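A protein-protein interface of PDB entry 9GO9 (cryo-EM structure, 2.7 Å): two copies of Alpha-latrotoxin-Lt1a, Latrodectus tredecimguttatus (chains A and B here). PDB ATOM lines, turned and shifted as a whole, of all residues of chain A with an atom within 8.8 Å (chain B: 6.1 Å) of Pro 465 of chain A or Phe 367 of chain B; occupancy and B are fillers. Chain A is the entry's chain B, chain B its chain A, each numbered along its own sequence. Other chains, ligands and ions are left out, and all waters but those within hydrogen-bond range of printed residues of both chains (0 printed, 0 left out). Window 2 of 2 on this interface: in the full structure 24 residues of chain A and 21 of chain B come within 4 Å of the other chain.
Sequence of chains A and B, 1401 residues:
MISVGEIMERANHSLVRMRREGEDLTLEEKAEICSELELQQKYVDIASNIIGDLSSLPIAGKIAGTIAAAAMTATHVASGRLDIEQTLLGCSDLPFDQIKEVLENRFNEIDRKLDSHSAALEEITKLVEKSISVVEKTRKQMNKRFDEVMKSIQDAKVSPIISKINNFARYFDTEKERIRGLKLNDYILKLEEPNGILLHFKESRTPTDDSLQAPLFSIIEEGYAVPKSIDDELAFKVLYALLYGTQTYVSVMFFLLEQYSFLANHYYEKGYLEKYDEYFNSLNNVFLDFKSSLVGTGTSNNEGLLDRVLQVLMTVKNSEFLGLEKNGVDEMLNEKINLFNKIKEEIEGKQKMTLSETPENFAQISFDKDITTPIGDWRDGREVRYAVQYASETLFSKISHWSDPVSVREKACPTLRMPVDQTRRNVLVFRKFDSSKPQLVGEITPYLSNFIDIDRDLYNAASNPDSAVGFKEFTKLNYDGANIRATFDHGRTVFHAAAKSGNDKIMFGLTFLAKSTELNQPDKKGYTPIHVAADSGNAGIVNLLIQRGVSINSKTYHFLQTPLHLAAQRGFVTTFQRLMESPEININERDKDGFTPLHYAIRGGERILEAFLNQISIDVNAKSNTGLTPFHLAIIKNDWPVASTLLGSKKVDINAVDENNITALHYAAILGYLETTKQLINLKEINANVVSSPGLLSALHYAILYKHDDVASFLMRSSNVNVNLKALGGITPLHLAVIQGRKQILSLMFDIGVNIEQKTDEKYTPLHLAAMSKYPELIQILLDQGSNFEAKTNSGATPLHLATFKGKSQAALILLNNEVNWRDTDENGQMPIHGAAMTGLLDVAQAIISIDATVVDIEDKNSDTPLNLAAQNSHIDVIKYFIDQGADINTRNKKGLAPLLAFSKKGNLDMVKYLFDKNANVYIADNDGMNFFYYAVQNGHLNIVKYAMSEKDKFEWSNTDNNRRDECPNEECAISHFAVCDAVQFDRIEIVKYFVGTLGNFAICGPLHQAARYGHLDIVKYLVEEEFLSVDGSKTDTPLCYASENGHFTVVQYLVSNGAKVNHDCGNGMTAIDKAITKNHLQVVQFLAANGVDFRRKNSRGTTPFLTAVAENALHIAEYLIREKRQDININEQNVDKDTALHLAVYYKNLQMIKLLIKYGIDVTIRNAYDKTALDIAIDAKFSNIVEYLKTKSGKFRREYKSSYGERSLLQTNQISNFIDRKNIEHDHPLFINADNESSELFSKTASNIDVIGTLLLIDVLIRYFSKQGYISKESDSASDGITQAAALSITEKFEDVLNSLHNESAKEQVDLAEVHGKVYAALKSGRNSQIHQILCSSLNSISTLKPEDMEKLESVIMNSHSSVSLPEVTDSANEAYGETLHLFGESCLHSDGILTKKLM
OD1 of Asp 368 of chain B sits at hydrogen-bond distance from OG of Ser 366 of chain B (2.7 Å).
The backbone carbonyl oxygen (O) of Ser 366 of chain B lies within hydrogen-bond range of the backbone NH (N) of Thr 415 of chain B, 2.9 Å away.
O of Val 406 of chain B sits at hydrogen-bond distance from N of Val 384 of chain B (3.1 Å).
O of Ala 462 of chain A is in hydrogen-bond range of OG of Ser 501 of chain A.
The backbone carbonyl oxygen (O) of Ala 497 of chain A lies within hydrogen-bond range of the side-chain hydroxyl (OG) of Ser 501 of chain A, at 3.3 Å.
No position is printed for both chains.
Of chain B, only Ser 366 (3.9 Å), Phe 367 (3.6 Å) and Val 406 (3.9 Å) come within 4 Å of Pro 465 of chain A.
Printed residues of chain B within 4 Å of Ser 501 of chain A: Gln 364 (3.7 Å).
Of the printed residues of chain A, Gln 364 of chain B touches Ser 501 (3.7 Å).
Of the printed residues of chain A, Ser 366 of chain B touches Pro 465.
Of chain A, only Pro 465 (3.6 Å) comes within 4 Å of Phe 367 of chain B.
Of the printed residues of chain A, Val 406 of chain B touches Pro 465.
Printed residues of chain A within 4 Å of Lys 411 of chain B: Asp 466.
The nearest printed residue of chain A that does not touch Gln 364 of chain B is Lys 500 of chain A (4.004 Å).
O of Pro 465 of chain A touches OG of Ser 366 of chain B (3.9 Å).
CB of Pro 465 of chain A touches CD2 of Phe 367 of chain B, 3.6 Å away.
Val 406 of chain B touches Pro 465 of chain A.
Ser 501 of chain A touches Gln 364 of chain B (O to OE1, 3.7 Å).
NZ of Lys 411 of chain B lies within salt-bridge range of OD1 of Asp 466 of chain A, 3.8 Å away.
Among the printed residues, 5 pairs touch across the chains.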
ATOM      1  N   ASN A 460      -2.827  -6.476  11.090  1.00  0.00           N
ATOM      2  CA  ASN A 460      -3.309  -7.848  10.968  1.00  0.00           C
ATOM      3  C   ASN A 460      -4.237  -8.001   9.770  1.00  0.00           C
ATOM      4  O   ASN A 460      -4.243  -9.049   9.113  1.00  0.00           O
ATOM      5  CB  ASN A 460      -4.015  -8.273  12.254  1.00  0.00           C
ATOM      6  CG  ASN A 460      -3.043  -8.626  13.362  1.00  0.00           C
ATOM      7  OD1 ASN A 460      -1.830  -8.648  13.155  1.00  0.00           O
ATOM      8  ND2 ASN A 460      -3.572  -8.904  14.548  1.00  0.00           N
ATOM      9  N   ALA A 461      -5.037  -6.973   9.477  1.00  0.00           N
ATOM     10  CA  ALA A 461      -5.920  -7.029   8.316  1.00  0.00           C
ATOM     11  C   ALA A 461      -5.123  -7.099   7.019  1.00  0.00           C
ATOM     12  O   ALA A 461      -5.506  -7.812   6.085  1.00  0.00           O
ATOM     13  CB  ALA A 461      -6.858  -5.823   8.307  1.00  0.00           C
ATOM     14  N   ALA A 462      -4.015  -6.359   6.941  1.00  0.00           N
ATOM     15  CA  ALA A 462      -3.171  -6.419   5.752  1.00  0.00           C
ATOM     16  C   ALA A 462      -2.478  -7.768   5.620  1.00  0.00           C
ATOM     17  O   ALA A 462      -2.088  -8.156   4.514  1.00  0.00           O
ATOM     18  CB  ALA A 462      -2.140  -5.291   5.780  1.00  0.00           C
ATOM     19  N   SER A 463      -2.315  -8.491   6.726  1.00  0.00           N
ATOM     20  CA  SER A 463      -1.690  -9.807   6.724  1.00  0.00           C
ATOM     21  C   SER A 463      -2.697 -10.938   6.564  1.00  0.00           C
ATOM     22  O   SER A 463      -2.311 -12.109   6.637  1.00  0.00           O
ATOM     23  CB  SER A 463      -0.886 -10.010   8.010  1.00  0.00           C
ATOM     24  OG  SER A 463       0.192  -9.093   8.091  1.00  0.00           O
ATOM     25  N   ASN A 464      -3.968 -10.618   6.356  1.00  0.00           N
ATOM     26  CA  ASN A 464      -4.992 -11.649   6.242  1.00  0.00           C
ATOM     27  C   ASN A 464      -4.778 -12.465   4.972  1.00  0.00           C
ATOM     28  O   ASN A 464      -4.664 -11.888   3.883  1.00  0.00           O
ATOM     29  CB  ASN A 464      -6.382 -11.014   6.234  1.00  0.00           C
ATOM     30  CG  ASN A 464      -7.476 -11.996   6.599  1.00  0.00           C
ATOM     31  OD1 ASN A 464      -7.227 -13.003   7.262  1.00  0.00           O
ATOM     32  ND2 ASN A 464      -8.697 -11.707   6.169  1.00  0.00           N
ATOM     33  N   PRO A 465      -4.704 -13.795   5.066  1.00  0.00           N
ATOM     34  CA  PRO A 465      -4.579 -14.607   3.844  1.00  0.00           C
ATOM     35  C   PRO A 465      -5.734 -14.422   2.876  1.00  0.00           C
ATOM     36  O   PRO A 465      -5.529 -14.507   1.659  1.00  0.00           O
ATOM     37  CB  PRO A 465      -4.517 -16.042   4.384  1.00  0.00           C
ATOM     38  CG  PRO A 465      -4.013 -15.896   5.782  1.00  0.00           C
ATOM     39  CD  PRO A 465      -4.600 -14.612   6.286  1.00  0.00           C
ATOM     40  N   ASP A 466      -6.941 -14.178   3.376  1.00  0.00           N
ATOM     41  CA  ASP A 466      -8.069 -13.898   2.501  1.00  0.00           C
ATOM     42  C   ASP A 466      -7.951 -12.493   1.919  1.00  0.00           C
ATOM     43  O   ASP A 466      -7.336 -11.600   2.509  1.00  0.00           O
ATOM     44  CB  ASP A 466      -9.386 -14.047   3.260  1.00  0.00           C
ATOM     45  CG  ASP A 466     -10.558 -14.336   2.344  1.00  0.00           C
ATOM     46  OD1 ASP A 466     -10.376 -14.285   1.110  1.00  0.00           O
ATOM     47  OD2 ASP A 466     -11.661 -14.615   2.857  1.00  0.00           O
ATOM     48  N   SER A 467      -8.551 -12.301   0.744  1.00  0.00           N
ATOM     49  CA  SER A 467      -8.446 -11.041   0.014  1.00  0.00           C
ATOM     50  C   SER A 467      -9.616 -10.107   0.305  1.00  0.00           C
ATOM     51  O   SER A 467      -9.411  -8.965   0.725  1.00  0.00           O
ATOM     52  CB  SER A 467      -8.343 -11.318  -1.492  1.00  0.00           C
ATOM     53  OG  SER A 467      -8.273 -10.109  -2.228  1.00  0.00           O
ATOM     54  N   ALA A 468     -10.847 -10.571   0.076  1.00  0.00           N
ATOM     55  CA  ALA A 468     -12.011  -9.712   0.276  1.00  0.00           C
ATOM     56  C   ALA A 468     -12.175  -9.329   1.742  1.00  0.00           C
ATOM     57  O   ALA A 468     -12.425  -8.159   2.060  1.00  0.00           O
ATOM     58  CB  ALA A 468     -13.269 -10.406  -0.242  1.00  0.00           C
ATOM     59  N   VAL A 469     -12.034 -10.299   2.647  1.00  0.00           N
ATOM     60  CA  VAL A 469     -12.194 -10.021   4.073  1.00  0.00           C
ATOM     61  C   VAL A 469     -11.135  -9.036   4.546  1.00  0.00           C
ATOM     62  O   VAL A 469     -11.431  -8.086   5.283  1.00  0.00           O
ATOM     63  CB  VAL A 469     -12.150 -11.334   4.879  1.00  0.00           C
ATOM     64  CG1 VAL A 469     -12.064 -11.046   6.369  1.00  0.00           C
ATOM     65  CG2 VAL A 469     -13.367 -12.189   4.563  1.00  0.00           C
ATOM     66  N   GLY A 470      -9.884  -9.246   4.130  1.00  0.00           N
ATOM     67  CA  GLY A 470      -8.825  -8.326   4.508  1.00  0.00           C
ATOM     68  C   GLY A 470      -9.056  -6.922   3.985  1.00  0.00           C
ATOM     69  O   GLY A 470      -8.834  -5.942   4.699  1.00  0.00           O
ATOM     70  N   PHE A 471      -9.508  -6.805   2.734  1.00  0.00           N
ATOM     71  CA  PHE A 471      -9.774  -5.489   2.161  1.00  0.00           C
ATOM     72  C   PHE A 471     -10.908  -4.783   2.896  1.00  0.00           C
ATOM     73  O   PHE A 471     -10.823  -3.579   3.176  1.00  0.00           O
ATOM     74  CB  PHE A 471     -10.098  -5.626   0.673  1.00  0.00           C
ATOM     75  CG  PHE A 471     -10.501  -4.337   0.016  1.00  0.00           C
ATOM     76  CD1 PHE A 471      -9.557  -3.366  -0.274  1.00  0.00           C
ATOM     77  CD2 PHE A 471     -11.824  -4.098  -0.318  1.00  0.00           C
ATOM     78  CE1 PHE A 471      -9.925  -2.180  -0.880  1.00  0.00           C
ATOM     79  CE2 PHE A 471     -12.197  -2.913  -0.924  1.00  0.00           C
ATOM     80  CZ  PHE A 471     -11.247  -1.954  -1.206  1.00  0.00           C
ATOM     81  N   GLU A 473     -11.862  -5.290   6.039  1.00  0.00           N
ATOM     82  CA  GLU A 473     -11.366  -4.893   7.352  1.00  0.00           C
ATOM     83  C   GLU A 473     -10.467  -3.668   7.249  1.00  0.00           C
ATOM     84  O   GLU A 473     -10.560  -2.748   8.071  1.00  0.00           O
ATOM     85  CB  GLU A 473     -10.622  -6.056   8.007  1.00  0.00           C
ATOM     86  CG  GLU A 473     -11.523  -7.201   8.440  1.00  0.00           C
ATOM     87  CD  GLU A 473     -10.750  -8.362   9.032  1.00  0.00           C
ATOM     88  OE1 GLU A 473      -9.509  -8.389   8.885  1.00  0.00           O
ATOM     89  OE2 GLU A 473     -11.381  -9.249   9.643  1.00  0.00           O
ATOM     90  N   ALA A 497       3.442  -5.762   5.594  1.00  0.00           N
ATOM     91  CA  ALA A 497       2.415  -6.772   5.832  1.00  0.00           C
ATOM     92  C   ALA A 497       1.631  -7.073   4.562  1.00  0.00           C
ATOM     93  O   ALA A 497       1.344  -8.237   4.263  1.00  0.00           O
ATOM     94  CB  ALA A 497       1.475  -6.312   6.946  1.00  0.00           C
ATOM     95  N   LYS A 500       3.867  -9.172   2.256  1.00  0.00           N
ATOM     96  CA  LYS A 500       3.978 -10.574   2.647  1.00  0.00           C
ATOM     97  C   LYS A 500       2.715 -11.352   2.296  1.00  0.00           C
ATOM     98  O   LYS A 500       2.794 -12.476   1.788  1.00  0.00           O
ATOM     99  CB  LYS A 500       4.280 -10.681   4.142  1.00  0.00           C
ATOM    100  CG  LYS A 500       4.026 -12.060   4.729  1.00  0.00           C
ATOM    101  CD  LYS A 500       4.939 -12.335   5.912  1.00  0.00           C
ATOM    102  CE  LYS A 500       6.288 -12.864   5.454  1.00  0.00           C
ATOM    103  NZ  LYS A 500       7.036 -13.516   6.564  1.00  0.00           N
ATOM    104  N   SER A 501       1.542 -10.770   2.553  1.00  0.00           N
ATOM    105  CA  SER A 501       0.294 -11.473   2.277  1.00  0.00           C
ATOM    106  C   SER A 501      -0.016 -11.514   0.786  1.00  0.00           C
ATOM    107  O   SER A 501      -0.640 -12.469   0.311  1.00  0.00           O
ATOM    108  CB  SER A 501      -0.860 -10.819   3.036  1.00  0.00           C
ATOM    109  OG  SER A 501      -1.111  -9.511   2.554  1.00  0.00           O
ATOM    110  N   GLY A 502       0.406 -10.499   0.036  1.00  0.00           N
ATOM    111  CA  GLY A 502       0.121 -10.457  -1.383  1.00  0.00           C
ATOM    112  C   GLY A 502      -1.240  -9.912  -1.743  1.00  0.00           C
ATOM    113  O   GLY A 502      -1.759 -10.226  -2.819  1.00  0.00           O
ATOM    114  N   ASN A 503      -1.840  -9.103  -0.873  1.00  0.00           N
ATOM    115  CA  ASN A 503      -3.134  -8.491  -1.151  1.00  0.00           C
ATOM    116  C   ASN A 503      -2.939  -7.361  -2.155  1.00  0.00           C
ATOM    117  O   ASN A 503      -2.346  -6.326  -1.829  1.00  0.00           O
ATOM    118  CB  ASN A 503      -3.769  -7.982   0.139  1.00  0.00           C
ATOM    119  CG  ASN A 503      -5.282  -8.053   0.112  1.00  0.00           C
ATOM    120  OD1 ASN A 503      -5.914  -7.712  -0.886  1.00  0.00           O
ATOM    121  ND2 ASN A 503      -5.873  -8.494   1.217  1.00  0.00           N
ATOM    122  N   ASN A 538       5.204 -13.406  -4.406  1.00  0.00           N
ATOM    123  CA  ASN A 538       4.112 -12.660  -5.012  1.00  0.00           C
ATOM    124  C   ASN A 538       4.589 -11.935  -6.267  1.00  0.00           C
ATOM    125  O   ASN A 538       5.743 -11.512  -6.366  1.00  0.00           O
ATOM    126  CB  ASN A 538       3.533 -11.658  -4.015  1.00  0.00           C
ATOM    127  CG  ASN A 538       2.680 -12.322  -2.954  1.00  0.00           C
ATOM    128  OD1 ASN A 538       1.553 -12.738  -3.218  1.00  0.00           O
ATOM    129  ND2 ASN A 538       3.216 -12.424  -1.744  1.00  0.00           N
ATOM    130  N   GLN B 364       4.511 -19.013   1.605  1.00  0.00           N
ATOM    131  CA  GLN B 364       3.342 -18.150   1.522  1.00  0.00           C
ATOM    132  C   GLN B 364       2.097 -19.024   1.460  1.00  0.00           C
ATOM    133  O   GLN B 364       2.116 -20.116   0.886  1.00  0.00           O
ATOM    134  CB  GLN B 364       3.433 -17.217   0.306  1.00  0.00           C
ATOM    135  CG  GLN B 364       2.361 -16.137   0.225  1.00  0.00           C
ATOM    136  CD  GLN B 364       1.087 -16.612  -0.440  1.00  0.00           C
ATOM    137  OE1 GLN B 364      -0.003 -16.126  -0.139  1.00  0.00           O
ATOM    138  NE2 GLN B 364       1.215 -17.578  -1.343  1.00  0.00           N
ATOM    139  N   ILE B 365       1.018 -18.539   2.070  1.00  0.00           N
ATOM    140  CA  ILE B 365      -0.251 -19.253   2.109  1.00  0.00           C
ATOM    141  C   ILE B 365      -1.364 -18.286   1.729  1.00  0.00           C
ATOM    142  O   ILE B 365      -1.333 -17.109   2.105  1.00  0.00           O
ATOM    143  CB  ILE B 365      -0.509 -19.888   3.495  1.00  0.00           C
ATOM    144  CG1 ILE B 365      -1.774 -20.750   3.469  1.00  0.00           C
ATOM    145  CG2 ILE B 365      -0.586 -18.822   4.582  1.00  0.00           C
ATOM    146  CD1 ILE B 365      -1.905 -21.673   4.658  1.00  0.00           C
ATOM    147  N   SER B 366      -2.334 -18.776   0.960  1.00  0.00           N
ATOM    148  CA  SER B 366      -3.439 -17.951   0.493  1.00  0.00           C
ATOM    149  C   SER B 366      -4.713 -18.787   0.478  1.00  0.00           C
ATOM    150  O   SER B 366      -4.705 -19.979   0.796  1.00  0.00           O
ATOM    151  CB  SER B 366      -3.145 -17.364  -0.891  1.00  0.00           C
ATOM    152  OG  SER B 366      -4.252 -16.627  -1.378  1.00  0.00           O
ATOM    153  N   PHE B 367      -5.822 -18.142   0.113  1.00  0.00           N
ATOM    154  CA  PHE B 367      -7.124 -18.795  -0.039  1.00  0.00           C
ATOM    155  C   PHE B 367      -7.699 -18.326  -1.371  1.00  0.00           C
ATOM    156  O   PHE B 367      -8.400 -17.312  -1.432  1.00  0.00           O
ATOM    157  CB  PHE B 367      -8.052 -18.468   1.128  1.00  0.00           C
ATOM    158  CG  PHE B 367      -7.679 -19.153   2.412  1.00  0.00           C
ATOM    159  CD1 PHE B 367      -8.188 -20.403   2.722  1.00  0.00           C
ATOM    160  CD2 PHE B 367      -6.822 -18.544   3.313  1.00  0.00           C
ATOM    161  CE1 PHE B 367      -7.849 -21.033   3.903  1.00  0.00           C
ATOM    162  CE2 PHE B 367      -6.478 -19.170   4.497  1.00  0.00           C
ATOM    163  CZ  PHE B 367      -6.992 -20.416   4.791  1.00  0.00           C
ATOM    164  N   ASP B 368      -7.402 -19.065  -2.439  1.00  0.00           N
ATOM    165  CA  ASP B 368      -7.792 -18.682  -3.790  1.00  0.00           C
ATOM    166  C   ASP B 368      -9.129 -19.280  -4.213  1.00  0.00           C
ATOM    167  O   ASP B 368      -9.967 -18.578  -4.783  1.00  0.00           O
ATOM    168  CB  ASP B 368      -6.701 -19.092  -4.785  1.00  0.00           C
ATOM    169  CG  ASP B 368      -5.310 -18.734  -4.303  1.00  0.00           C
ATOM    170  OD1 ASP B 368      -5.155 -17.674  -3.661  1.00  0.00           O
ATOM    171  OD2 ASP B 368      -4.368 -19.512  -4.566  1.00  0.00           O
ATOM    172  N   LYS B 369      -9.343 -20.567  -3.951  1.00  0.00           N
ATOM    173  CA  LYS B 369     -10.584 -21.213  -4.354  1.00  0.00           C
ATOM    174  C   LYS B 369     -11.762 -20.663  -3.560  1.00  0.00           C
ATOM    175  O   LYS B 369     -11.673 -20.451  -2.347  1.00  0.00           O
ATOM    176  CB  LYS B 369     -10.483 -22.726  -4.164  1.00  0.00           C
ATOM    177  CG  LYS B 369      -9.497 -23.399  -5.103  1.00  0.00           C
ATOM    178  CD  LYS B 369      -9.487 -24.905  -4.908  1.00  0.00           C
ATOM    179  CE  LYS B 369      -8.450 -25.567  -5.799  1.00  0.00           C
ATOM    180  NZ  LYS B 369      -8.810 -25.457  -7.240  1.00  0.00           N
ATOM    181  N   TRP B 378     -12.745 -27.655   8.420  1.00  0.00           N
ATOM    182  CA  TRP B 378     -12.612 -26.209   8.290  1.00  0.00           C
ATOM    183  C   TRP B 378     -13.860 -25.545   8.858  1.00  0.00           C
ATOM    184  O   TRP B 378     -14.937 -25.614   8.257  1.00  0.00           O
ATOM    185  CB  TRP B 378     -12.401 -25.822   6.829  1.00  0.00           C
ATOM    186  CG  TRP B 378     -11.210 -26.465   6.189  1.00  0.00           C
ATOM    187  CD1 TRP B 378     -11.200 -27.590   5.420  1.00  0.00           C
ATOM    188  CD2 TRP B 378      -9.853 -26.010   6.251  1.00  0.00           C
ATOM    189  NE1 TRP B 378      -9.921 -27.869   5.004  1.00  0.00           N
ATOM    190  CE2 TRP B 378      -9.075 -26.914   5.501  1.00  0.00           C
ATOM    191  CE3 TRP B 378      -9.219 -24.928   6.870  1.00  0.00           C
ATOM    192  CZ2 TRP B 378      -7.698 -26.769   5.353  1.00  0.00           C
ATOM    193  CZ3 TRP B 378      -7.852 -24.786   6.723  1.00  0.00           C
ATOM    194  CH2 TRP B 378      -7.106 -25.701   5.971  1.00  0.00           C
ATOM    195  N   VAL B 384      -5.226 -23.548  11.969  1.00  0.00           N
ATOM    196  CA  VAL B 384      -4.600 -24.632  11.221  1.00  0.00           C
ATOM    197  C   VAL B 384      -3.090 -24.434  11.237  1.00  0.00           C
ATOM    198  O   VAL B 384      -2.602 -23.302  11.135  1.00  0.00           O
ATOM    199  CB  VAL B 384      -5.137 -24.714   9.777  1.00  0.00           C
ATOM    200  CG1 VAL B 384      -4.786 -23.462   8.984  1.00  0.00           C
ATOM    201  CG2 VAL B 384      -4.614 -25.959   9.080  1.00  0.00           C
ATOM    202  N   VAL B 406      -3.091 -20.153  11.500  1.00  0.00           N
ATOM    203  CA  VAL B 406      -3.820 -19.421  10.472  1.00  0.00           C
ATOM    204  C   VAL B 406      -5.307 -19.537  10.772  1.00  0.00           C
ATOM    205  O   VAL B 406      -5.831 -20.647  10.913  1.00  0.00           O
ATOM    206  CB  VAL B 406      -3.510 -19.951   9.058  1.00  0.00           C
ATOM    207  CG1 VAL B 406      -4.221 -19.111   8.009  1.00  0.00           C
ATOM    208  CG2 VAL B 406      -2.009 -19.963   8.812  1.00  0.00           C
ATOM    209  N   SER B 407      -5.981 -18.396  10.872  1.00  0.00           N
ATOM    210  CA  SER B 407      -7.404 -18.391  11.177  1.00  0.00           C
ATOM    211  C   SER B 407      -8.222 -18.774   9.948  1.00  0.00           C
ATOM    212  O   SER B 407      -7.822 -18.536   8.806  1.00  0.00           O
ATOM    213  CB  SER B 407      -7.833 -17.017  11.687  1.00  0.00           C
ATOM    214  OG  SER B 407      -7.710 -16.036  10.672  1.00  0.00           O
ATOM    215  N   VAL B 408      -9.385 -19.371  10.195  1.00  0.00           N
ATOM    216  CA  VAL B 408     -10.285 -19.827   9.142  1.00  0.00           C
ATOM    217  C   VAL B 408     -11.528 -18.949   9.183  1.00  0.00           C
ATOM    218  O   VAL B 408     -12.301 -18.996  10.148  1.00  0.00           O
ATOM    219  CB  VAL B 408     -10.647 -21.309   9.304  1.00  0.00           C
ATOM    220  CG1 VAL B 408     -11.596 -21.747   8.200  1.00  0.00           C
ATOM    221  CG2 VAL B 408      -9.390 -22.166   9.308  1.00  0.00           C
ATOM    222  N   LYS B 411     -13.356 -19.181   4.214  1.00  0.00           N
ATOM    223  CA  LYS B 411     -12.601 -19.891   3.192  1.00  0.00           C
ATOM    224  C   LYS B 411     -12.081 -21.196   3.771  1.00  0.00           C
ATOM    225  O   LYS B 411     -11.627 -21.235   4.918  1.00  0.00           O
ATOM    226  CB  LYS B 411     -11.439 -19.044   2.661  1.00  0.00           C
ATOM    227  CG  LYS B 411     -11.853 -17.990   1.646  1.00  0.00           C
ATOM    228  CD  LYS B 411     -12.693 -18.593   0.533  1.00  0.00           C
ATOM    229  CE  LYS B 411     -13.151 -17.528  -0.450  1.00  0.00           C
ATOM    230  NZ  LYS B 411     -12.003 -16.877  -1.138  1.00  0.00           N
ATOM    231  N   ALA B 412     -12.144 -22.262   2.973  1.00  0.00           N
ATOM    232  CA  ALA B 412     -11.810 -23.602   3.439  1.00  0.00           C
ATOM    233  C   ALA B 412     -10.477 -24.101   2.897  1.00  0.00           C
ATOM    234  O   ALA B 412      -9.590 -24.459   3.676  1.00  0.00           O
ATOM    235  CB  ALA B 412     -12.935 -24.577   3.064  1.00  0.00           C
ATOM    236  N   CYS B 413     -10.304 -24.132   1.575  1.00  0.00           N
ATOM    237  CA  CYS B 413      -9.144 -24.779   0.977  1.00  0.00           C
ATOM    238  C   CYS B 413      -8.062 -23.753   0.688  1.00  0.00           C
ATOM    239  O   CYS B 413      -8.273 -22.865  -0.152  1.00  0.00           O
ATOM    240  CB  CYS B 413      -9.539 -25.503  -0.304  1.00  0.00           C
ATOM    241  SG  CYS B 413     -10.571 -26.961  -0.035  1.00  0.00           S
ATOM    242  N   PRO B 414      -6.906 -23.830   1.342  1.00  0.00           N
ATOM    243  CA  PRO B 414      -5.823 -22.886   1.068  1.00  0.00           C
ATOM    244  C   PRO B 414      -4.855 -23.402   0.012  1.00  0.00           C
ATOM    245  O   PRO B 414      -4.830 -24.584  -0.334  1.00  0.00           O
ATOM    246  CB  PRO B 414      -5.128 -22.771   2.431  1.00  0.00           C
ATOM    247  CG  PRO B 414      -5.297 -24.136   3.029  1.00  0.00           C
ATOM    248  CD  PRO B 414      -6.579 -24.727   2.464  1.00  0.00           C
ATOM    249  N   THR B 415      -4.049 -22.476  -0.497  1.00  0.00           N
ATOM    250  CA  THR B 415      -2.976 -22.780  -1.434  1.00  0.00           C
ATOM    251  C   THR B 415      -1.646 -22.395  -0.804  1.00  0.00           C
ATOM    252  O   THR B 415      -1.500 -21.285  -0.281  1.00  0.00           O
ATOM    253  CB  THR B 415      -3.170 -22.040  -2.760  1.00  0.00           C
ATOM    254  OG1 THR B 415      -4.539 -22.143  -3.171  1.00  0.00           O
ATOM    255  CG2 THR B 415      -2.277 -22.636  -3.837  1.00  0.00           C
